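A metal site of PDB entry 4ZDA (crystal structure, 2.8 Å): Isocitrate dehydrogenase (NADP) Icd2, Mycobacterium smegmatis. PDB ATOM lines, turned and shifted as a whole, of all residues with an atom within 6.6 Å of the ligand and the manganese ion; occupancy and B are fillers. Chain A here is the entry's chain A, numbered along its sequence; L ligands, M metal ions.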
ATOM      1  N   SER A  89      -1.870   4.960 -18.208  1.00  0.00           N
ATOM      2  CA  SER A  89      -0.663   4.478 -17.540  1.00  0.00           C
ATOM      3  C   SER A  89       0.449   5.510 -17.760  1.00  0.00           C
ATOM      4  O   SER A  89       1.242   5.387 -18.692  1.00  0.00           O
ATOM      5  CB  SER A  89      -0.244   3.103 -18.057  1.00  0.00           C
ATOM      6  OG  SER A  89      -0.861   2.088 -17.299  1.00  0.00           O
ATOM      7  N   SER A 134       2.113   1.369 -15.121  1.00  0.00           N
ATOM      8  CA  SER A 134       0.938   0.515 -14.934  1.00  0.00           C
ATOM      9  C   SER A 134       0.645   0.306 -13.445  1.00  0.00           C
ATOM     10  O   SER A 134       1.087  -0.668 -12.831  1.00  0.00           O
ATOM     11  CB  SER A 134       1.141  -0.818 -15.645  1.00  0.00           C
ATOM     12  OG  SER A 134      -0.046  -1.595 -15.605  1.00  0.00           O
ATOM     13  N   ASN A 137      -4.149  -1.622 -12.876  1.00  0.00           N
ATOM     14  CA  ASN A 137      -4.397  -3.048 -13.092  1.00  0.00           C
ATOM     15  C   ASN A 137      -3.847  -3.990 -12.008  1.00  0.00           C
ATOM     16  O   ASN A 137      -4.548  -4.936 -11.625  1.00  0.00           O
ATOM     17  CB  ASN A 137      -3.898  -3.498 -14.479  1.00  0.00           C
ATOM     18  CG  ASN A 137      -4.775  -2.975 -15.610  1.00  0.00           C
ATOM     19  OD1 ASN A 137      -5.855  -2.438 -15.387  1.00  0.00           O
ATOM     20  ND2 ASN A 137      -4.292  -3.142 -16.840  1.00  0.00           N
ATOM     21  N   PRO A 138      -2.621  -3.765 -11.511  1.00  0.00           N
ATOM     22  CA  PRO A 138      -2.140  -4.698 -10.491  1.00  0.00           C
ATOM     23  C   PRO A 138      -2.956  -4.674  -9.201  1.00  0.00           C
ATOM     24  O   PRO A 138      -2.918  -5.639  -8.431  1.00  0.00           O
ATOM     25  CB  PRO A 138      -0.704  -4.219 -10.214  1.00  0.00           C
ATOM     26  CG  PRO A 138      -0.322  -3.430 -11.411  1.00  0.00           C
ATOM     27  CD  PRO A 138      -1.585  -2.757 -11.835  1.00  0.00           C
ATOM     28  N   ARG A 141      -6.930  -6.258 -10.411  1.00  0.00           N
ATOM     29  CA  ARG A 141      -7.005  -7.623 -10.937  1.00  0.00           C
ATOM     30  C   ARG A 141      -6.843  -8.674  -9.835  1.00  0.00           C
ATOM     31  O   ARG A 141      -5.756  -9.250  -9.650  1.00  0.00           O
ATOM     32  CB  ARG A 141      -6.036  -7.816 -12.099  1.00  0.00           C
ATOM     33  CG  ARG A 141      -6.470  -7.046 -13.335  1.00  0.00           C
ATOM     34  CD  ARG A 141      -5.432  -7.027 -14.446  1.00  0.00           C
ATOM     35  NE  ARG A 141      -6.007  -6.476 -15.672  1.00  0.00           N
ATOM     36  CZ  ARG A 141      -5.369  -6.392 -16.837  1.00  0.00           C
ATOM     37  NH1 ARG A 141      -4.121  -6.821 -16.938  1.00  0.00           N
ATOM     38  NH2 ARG A 141      -5.971  -5.879 -17.895  1.00  0.00           N
ATOM     39  N   ARG A 147     -12.129 -13.075 -21.249  1.00  0.00           N
ATOM     40  CA  ARG A 147     -12.186 -12.114 -22.339  1.00  0.00           C
ATOM     41  C   ARG A 147     -12.646 -12.813 -23.610  1.00  0.00           C
ATOM     42  O   ARG A 147     -12.069 -13.824 -24.015  1.00  0.00           O
ATOM     43  CB  ARG A 147     -10.812 -11.438 -22.523  1.00  0.00           C
ATOM     44  CG  ARG A 147     -10.912  -9.999 -23.013  1.00  0.00           C
ATOM     45  CD  ARG A 147      -9.602  -9.218 -22.864  1.00  0.00           C
ATOM     46  NE  ARG A 147      -9.187  -9.066 -21.470  1.00  0.00           N
ATOM     47  CZ  ARG A 147      -8.199  -8.258 -21.048  1.00  0.00           C
ATOM     48  NH1 ARG A 147      -7.513  -7.518 -21.909  1.00  0.00           N
ATOM     49  NH2 ARG A 147      -7.914  -8.203 -19.758  1.00  0.00           N
ATOM     50  N   LYS A 257       7.343  -4.943 -24.605  1.00  0.00           N
ATOM     51  CA  LYS A 257       6.306  -4.385 -23.754  1.00  0.00           C
ATOM     52  C   LYS A 257       6.951  -3.560 -22.635  1.00  0.00           C
ATOM     53  O   LYS A 257       6.904  -3.936 -21.457  1.00  0.00           O
ATOM     54  CB  LYS A 257       5.427  -5.516 -23.200  1.00  0.00           C
ATOM     55  CG  LYS A 257       4.246  -5.092 -22.359  1.00  0.00           C
ATOM     56  CD  LYS A 257       2.932  -5.087 -23.135  1.00  0.00           C
ATOM     57  CE  LYS A 257       1.757  -5.016 -22.182  1.00  0.00           C
ATOM     58  NZ  LYS A 257       0.463  -5.121 -22.908  1.00  0.00           N
ATOM     59  N   THR A 259       6.340  -0.516 -21.270  1.00  0.00           N
ATOM     60  CA  THR A 259       5.492   0.145 -20.273  1.00  0.00           C
ATOM     61  C   THR A 259       5.237  -0.743 -19.064  1.00  0.00           C
ATOM     62  O   THR A 259       5.525  -0.356 -17.935  1.00  0.00           O
ATOM     63  CB  THR A 259       4.127   0.556 -20.856  1.00  0.00           C
ATOM     64  OG1 THR A 259       4.304   1.057 -22.187  1.00  0.00           O
ATOM     65  CG2 THR A 259       3.469   1.641 -19.968  1.00  0.00           C
ATOM     66  N   MET A 260       4.712  -1.939 -19.318  1.00  0.00           N
ATOM     67  CA  MET A 260       4.348  -2.861 -18.243  1.00  0.00           C
ATOM     68  C   MET A 260       5.591  -3.551 -17.656  1.00  0.00           C
ATOM     69  O   MET A 260       5.785  -3.548 -16.446  1.00  0.00           O
ATOM     70  CB  MET A 260       3.305  -3.867 -18.740  1.00  0.00           C
ATOM     71  CG  MET A 260       2.711  -4.765 -17.662  1.00  0.00           C
ATOM     72  SD  MET A 260       3.728  -6.227 -17.341  1.00  0.00           S
ATOM     73  CE  MET A 260       3.554  -7.090 -18.913  1.00  0.00           C
ATOM     74  N   MET A 261       6.414  -4.134 -18.533  1.00  0.00           N
ATOM     75  CA  MET A 261       7.683  -4.730 -18.100  1.00  0.00           C
ATOM     76  C   MET A 261       8.716  -3.622 -17.914  1.00  0.00           C
ATOM     77  O   MET A 261       9.629  -3.463 -18.719  1.00  0.00           O
ATOM     78  CB  MET A 261       8.184  -5.773 -19.116  1.00  0.00           C
ATOM     79  CG  MET A 261       7.176  -6.858 -19.470  1.00  0.00           C
ATOM     80  SD  MET A 261       6.778  -8.011 -18.141  1.00  0.00           S
ATOM     81  CE  MET A 261       8.259  -9.024 -18.107  1.00  0.00           C
ATOM     82  N   ILE A 350       4.561  -1.368 -28.952  1.00  0.00           N
ATOM     83  CA  ILE A 350       4.236  -2.302 -27.867  1.00  0.00           C
ATOM     84  C   ILE A 350       3.773  -3.630 -28.456  1.00  0.00           C
ATOM     85  O   ILE A 350       2.803  -3.669 -29.220  1.00  0.00           O
ATOM     86  CB  ILE A 350       3.150  -1.735 -26.907  1.00  0.00           C
ATOM     87  CG1 ILE A 350       3.528  -0.346 -26.383  1.00  0.00           C
ATOM     88  CG2 ILE A 350       2.963  -2.658 -25.712  1.00  0.00           C
ATOM     89  CD1 ILE A 350       2.729   0.774 -27.001  1.00  0.00           C
ATOM     90  N   ASP A 352       1.967  -6.342 -27.841  1.00  0.00           N
ATOM     91  CA  ASP A 352       0.594  -6.819 -27.918  1.00  0.00           C
ATOM     92  C   ASP A 352      -0.255  -6.124 -28.970  1.00  0.00           C
ATOM     93  O   ASP A 352      -1.190  -6.707 -29.496  1.00  0.00           O
ATOM     94  CB  ASP A 352      -0.093  -6.841 -26.536  1.00  0.00           C
ATOM     95  CG  ASP A 352      -0.235  -5.448 -25.916  1.00  0.00           C
ATOM     96  OD1 ASP A 352       0.626  -4.574 -26.138  1.00  0.00           O
ATOM     97  OD2 ASP A 352      -1.218  -5.235 -25.174  1.00  0.00           O
ATOM     98  N   ALA A 353       0.082  -4.871 -29.278  1.00  0.00           N
ATOM     99  CA  ALA A 353      -0.676  -4.094 -30.267  1.00  0.00           C
ATOM    100  C   ALA A 353      -0.003  -4.086 -31.623  1.00  0.00           C
ATOM    101  O   ALA A 353      -0.664  -4.108 -32.667  1.00  0.00           O
ATOM    102  CB  ALA A 353      -0.899  -2.675 -29.777  1.00  0.00           C
ATOM    103  N   MET A 415      -4.410 -14.538 -14.309  1.00  0.00           N
ATOM    104  CA  MET A 415      -3.856 -13.211 -14.037  1.00  0.00           C
ATOM    105  C   MET A 415      -4.019 -12.706 -12.597  1.00  0.00           C
ATOM    106  O   MET A 415      -3.452 -11.667 -12.235  1.00  0.00           O
ATOM    107  CB  MET A 415      -4.422 -12.177 -15.013  1.00  0.00           C
ATOM    108  CG  MET A 415      -5.874 -11.822 -14.778  1.00  0.00           C
ATOM    109  SD  MET A 415      -6.357 -10.379 -15.732  1.00  0.00           S
ATOM    110  CE  MET A 415      -8.005 -10.085 -15.088  1.00  0.00           C
ATOM    111  N   TYR A 422       3.739 -10.455 -14.433  1.00  0.00           N
ATOM    112  CA  TYR A 422       3.111  -9.189 -14.065  1.00  0.00           C
ATOM    113  C   TYR A 422       3.383  -8.759 -12.626  1.00  0.00           C
ATOM    114  O   TYR A 422       3.000  -7.669 -12.211  1.00  0.00           O
ATOM    115  CB  TYR A 422       1.593  -9.269 -14.302  1.00  0.00           C
ATOM    116  CG  TYR A 422       1.189  -9.030 -15.739  1.00  0.00           C
ATOM    117  CD1 TYR A 422       1.561  -9.910 -16.747  1.00  0.00           C
ATOM    118  CD2 TYR A 422       0.428  -7.915 -16.082  1.00  0.00           C
ATOM    119  CE1 TYR A 422       1.187  -9.692 -18.061  1.00  0.00           C
ATOM    120  CE2 TYR A 422       0.046  -7.681 -17.400  1.00  0.00           C
ATOM    121  CZ  TYR A 422       0.438  -8.578 -18.383  1.00  0.00           C
ATOM    122  OH  TYR A 422       0.069  -8.368 -19.686  1.00  0.00           O
ATOM    123  N   ASN A 547      -0.606 -15.472 -17.957  1.00  0.00           N
ATOM    124  CA  ASN A 547      -0.852 -14.038 -17.915  1.00  0.00           C
ATOM    125  C   ASN A 547      -0.468 -13.304 -19.203  1.00  0.00           C
ATOM    126  O   ASN A 547      -1.282 -12.582 -19.772  1.00  0.00           O
ATOM    127  CB  ASN A 547      -0.146 -13.406 -16.716  1.00  0.00           C
ATOM    128  CG  ASN A 547      -0.872 -12.191 -16.174  1.00  0.00           C
ATOM    129  OD1 ASN A 547      -1.722 -11.598 -16.843  1.00  0.00           O
ATOM    130  ND2 ASN A 547      -0.534 -11.806 -14.937  1.00  0.00           N
ATOM    131  N   ARG A 550      -2.402 -14.294 -22.250  1.00  0.00           N
ATOM    132  CA  ARG A 550      -3.733 -13.686 -22.113  1.00  0.00           C
ATOM    133  C   ARG A 550      -3.734 -12.323 -22.790  1.00  0.00           C
ATOM    134  O   ARG A 550      -4.598 -12.024 -23.599  1.00  0.00           O
ATOM    135  CB  ARG A 550      -4.114 -13.551 -20.633  1.00  0.00           C
ATOM    136  CG  ARG A 550      -5.258 -12.590 -20.332  1.00  0.00           C
ATOM    137  CD  ARG A 550      -5.078 -11.964 -18.955  1.00  0.00           C
ATOM    138  NE  ARG A 550      -3.827 -11.225 -18.855  1.00  0.00           N
ATOM    139  CZ  ARG A 550      -3.690  -9.918 -19.078  1.00  0.00           C
ATOM    140  NH1 ARG A 550      -4.738  -9.164 -19.397  1.00  0.00           N
ATOM    141  NH2 ARG A 550      -2.498  -9.358 -18.970  1.00  0.00           N
ATOM    142  N   ASP A 551      -2.718 -11.523 -22.456  1.00  0.00           N
ATOM    143  CA  ASP A 551      -2.498 -10.208 -23.022  1.00  0.00           C
ATOM    144  C   ASP A 551      -2.373 -10.265 -24.552  1.00  0.00           C
ATOM    145  O   ASP A 551      -3.127  -9.589 -25.264  1.00  0.00           O
ATOM    146  CB  ASP A 551      -1.229  -9.592 -22.421  1.00  0.00           C
ATOM    147  CG  ASP A 551      -0.955  -8.178 -22.910  1.00  0.00           C
ATOM    148  OD1 ASP A 551      -1.896  -7.468 -23.327  1.00  0.00           O
ATOM    149  OD2 ASP A 551       0.229  -7.773 -22.849  1.00  0.00           O
ATOM    150  N   TYR A 552      -1.438 -11.091 -25.038  1.00  0.00           N
ATOM    151  CA  TYR A 552      -1.155 -11.182 -26.463  1.00  0.00           C
ATOM    152  C   TYR A 552      -2.373 -11.635 -27.254  1.00  0.00           C
ATOM    153  O   TYR A 552      -2.805 -10.945 -28.177  1.00  0.00           O
ATOM    154  CB  TYR A 552       0.027 -12.127 -26.723  1.00  0.00           C
ATOM    155  CG  TYR A 552       1.403 -11.601 -26.351  1.00  0.00           C
ATOM    156  CD1 TYR A 552       1.552 -10.480 -25.521  1.00  0.00           C
ATOM    157  CD2 TYR A 552       2.557 -12.254 -26.787  1.00  0.00           C
ATOM    158  CE1 TYR A 552       2.816 -10.028 -25.167  1.00  0.00           C
ATOM    159  CE2 TYR A 552       3.813 -11.800 -26.437  1.00  0.00           C
ATOM    160  CZ  TYR A 552       3.937 -10.683 -25.626  1.00  0.00           C
ATOM    161  OH  TYR A 552       5.189 -10.236 -25.270  1.00  0.00           O
ATOM    162  N   THR A 554      -5.602 -11.889 -26.664  1.00  0.00           N
ATOM    163  CA  THR A 554      -6.831 -11.105 -26.608  1.00  0.00           C
ATOM    164  C   THR A 554      -6.712  -9.829 -27.422  1.00  0.00           C
ATOM    165  O   THR A 554      -7.692  -9.108 -27.609  1.00  0.00           O
ATOM    166  CB  THR A 554      -7.247 -10.751 -25.164  1.00  0.00           C
ATOM    167  OG1 THR A 554      -6.150 -10.112 -24.495  1.00  0.00           O
ATOM    168  CG2 THR A 554      -7.635 -11.990 -24.405  1.00  0.00           C
ATOM    169  N   ASP A 555      -5.509  -9.533 -27.887  1.00  0.00           N
ATOM    170  CA  ASP A 555      -5.307  -8.488 -28.891  1.00  0.00           C
ATOM    171  C   ASP A 555      -5.291  -9.120 -30.287  1.00  0.00           C
ATOM    172  O   ASP A 555      -5.951  -8.634 -31.201  1.00  0.00           O
ATOM    173  CB  ASP A 555      -4.034  -7.692 -28.634  1.00  0.00           C
ATOM    174  CG  ASP A 555      -4.282  -6.429 -27.819  1.00  0.00           C
ATOM    175  OD1 ASP A 555      -4.890  -5.481 -28.368  1.00  0.00           O
ATOM    176  OD2 ASP A 555      -3.865  -6.377 -26.647  1.00  0.00           O
ATOM    177  N   SER A 565      -9.738  -4.408 -30.692  1.00  0.00           N
ATOM    178  CA  SER A 565      -9.917  -5.120 -29.436  1.00  0.00           C
ATOM    179  C   SER A 565     -10.846  -4.335 -28.494  1.00  0.00           C
ATOM    180  O   SER A 565     -11.089  -4.760 -27.359  1.00  0.00           O
ATOM    181  CB  SER A 565      -8.574  -5.446 -28.756  1.00  0.00           C
ATOM    182  OG  SER A 565      -8.110  -4.380 -27.928  1.00  0.00           O
ATOM    183  N   GLU A 582     -13.913  -4.817 -17.081  1.00  0.00           N
ATOM    184  CA  GLU A 582     -13.093  -3.916 -17.876  1.00  0.00           C
ATOM    185  C   GLU A 582     -13.782  -3.656 -19.218  1.00  0.00           C
ATOM    186  O   GLU A 582     -14.050  -4.589 -19.959  1.00  0.00           O
ATOM    187  CB  GLU A 582     -11.689  -4.487 -18.089  1.00  0.00           C
ATOM    188  CG  GLU A 582     -10.870  -4.659 -16.813  1.00  0.00           C
ATOM    189  CD  GLU A 582      -9.612  -5.500 -16.994  1.00  0.00           C
ATOM    190  OE1 GLU A 582      -8.631  -5.269 -16.252  1.00  0.00           O
ATOM    191  OE2 GLU A 582      -9.584  -6.404 -17.864  1.00  0.00           O
ATOM    192  N   GLY A 584     -12.622  -1.790 -21.746  1.00  0.00           N
ATOM    193  CA  GLY A 584     -11.649  -1.779 -22.840  1.00  0.00           C
ATOM    194  C   GLY A 584     -10.277  -2.230 -22.378  1.00  0.00           C
ATOM    195  O   GLY A 584      -9.952  -2.162 -21.194  1.00  0.00           O
ATOM    196  N   ALA A 585      -9.461  -2.683 -23.324  1.00  0.00           N
ATOM    197  CA  ALA A 585      -8.124  -3.168 -23.033  1.00  0.00           C
ATOM    198  C   ALA A 585      -7.040  -2.225 -23.527  1.00  0.00           C
ATOM    199  O   ALA A 585      -5.843  -2.478 -23.353  1.00  0.00           O
ATOM    200  CB  ALA A 585      -7.920  -4.553 -23.640  1.00  0.00           C
ATOM    201  N   GLY A 586      -7.455  -1.118 -24.140  1.00  0.00           N
ATOM    202  CA  GLY A 586      -6.513  -0.212 -24.793  1.00  0.00           C
ATOM    203  C   GLY A 586      -6.314   1.106 -24.068  1.00  0.00           C
ATOM    204  O   GLY A 586      -6.365   1.170 -22.840  1.00  0.00           O
HETATM  205  C1  LIG L   1      -4.420  -4.944 -21.749  1.00  0.00           C
HETATM  206  O1  LIG L   1      -4.647  -5.149 -22.962  1.00  0.00           O
HETATM  207  O2  LIG L   1      -5.123  -5.420 -20.832  1.00  0.00           O
HETATM  208  C2  LIG L   1      -3.238  -4.076 -21.419  1.00  0.00           C
HETATM  209  O3  LIG L   1      -2.189  -4.333 -22.363  1.00  0.00           O
HETATM  210  C3  LIG L   1      -2.735  -4.290 -19.976  1.00  0.00           C
HETATM  211  C4  LIG L   1      -1.806  -3.126 -19.597  1.00  0.00           C
HETATM  212  C5  LIG L   1      -1.059  -3.320 -18.292  1.00  0.00           C
HETATM  213  O4  LIG L   1      -1.614  -3.836 -17.298  1.00  0.00           O
HETATM  214  O5  LIG L   1       0.119  -2.913 -18.265  1.00  0.00           O
HETATM  215  C6  LIG L   1      -2.121  -5.662 -19.811  1.00  0.00           C
HETATM  216  O6  LIG L   1      -2.818  -6.555 -19.303  1.00  0.00           O
HETATM  217  O7  LIG L   1      -0.954  -5.883 -20.211  1.00  0.00           O
HETATM  218 MN    MN M   1      -3.315  -5.999 -24.168  1.00  0.00          MN
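The side-chain carboxylate of Asp 551 is in hydrogen-bond range of the side-chain hydroxyl of Tyr 422 (3.2 Å).
O of Asp 551 is in hydrogen-bond range of OG1 of Thr 554, at 3.2 Å.
The side-chain carboxylate (OD1) of Asp 352 is in salt-bridge range of the side-chain amino group (NZ) of Lys 257, at 3.3 Å.
The side-chain hydroxyl of Ser 565 is in hydrogen-bond range of the side-chain carboxylate of Asp 555, 3.4 Å away.
NE of Arg 141 is in salt-bridge range of OE1 of Glu 582.
The side-chain hydroxyl of Tyr 422 is in hydrogen-bond range of the guanidinium group of Arg 550, 2.8 Å away.
The side-chain amide oxygen (OD1) of Asn 547 sits at hydrogen-bond distance from the guanidinium group (NE) of Arg 550, at 2.9 Å.
The guanidinium group of Arg 147 lies within salt-bridge range of the side-chain carboxylate of Glu 582, at 3.1 Å.
The manganese ion is bound by O1 of the ligand (2.0 Å), OD1 of Asp 551 (2.2 Å), OD2 of Asp 352 (2.4 Å) and OD2 of Asp 555 (2.6 Å).
The manganese ion has four donor atoms within binding distance.
Slightly farther from the manganese ion lies O3 of the ligand (2.7 Å).
Of the 26 residues printed, 3 come within 4 Å of the manganese ion.
The nearest printed residue that does not touch the manganese ion is Lys 257 (4.1 Å).
The guanidinium group of Arg 141 is in salt-bridge range of an oxygen (O6) of the ligand (2.7 Å).
The side-chain hydroxyl (OH) of Tyr 422 is in hydrogen-bond range of an oxygen (O7) of the ligand (2.7 Å).
ND2 of Asn 137 lies within hydrogen-bond range of O4 of the ligand (2.8 Å).
NZ of Lys 257 is in salt-bridge range of O7 of the ligand (3.1 Å).
An oxygen (O6) of the ligand is in salt-bridge range of the guanidinium group (NH2) of Arg 550.
An oxygen (O5) of the ligand lies within hydrogen-bond range of the side-chain hydroxyl of Ser 134 (3.0 Å).
The guanidinium group of Arg 147 is in salt-bridge range of an oxygen (O2) of the ligand, at 3.4 Å.
The backbone carbonyl oxygen (O) of Ala 585 sits close to an oxygen (O1) of the ligand.
CG of Met 260 touches O5 of the ligand, 3.2 Å away.
Of the 26 residues printed, 12 come within 4 Å of the ligand.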
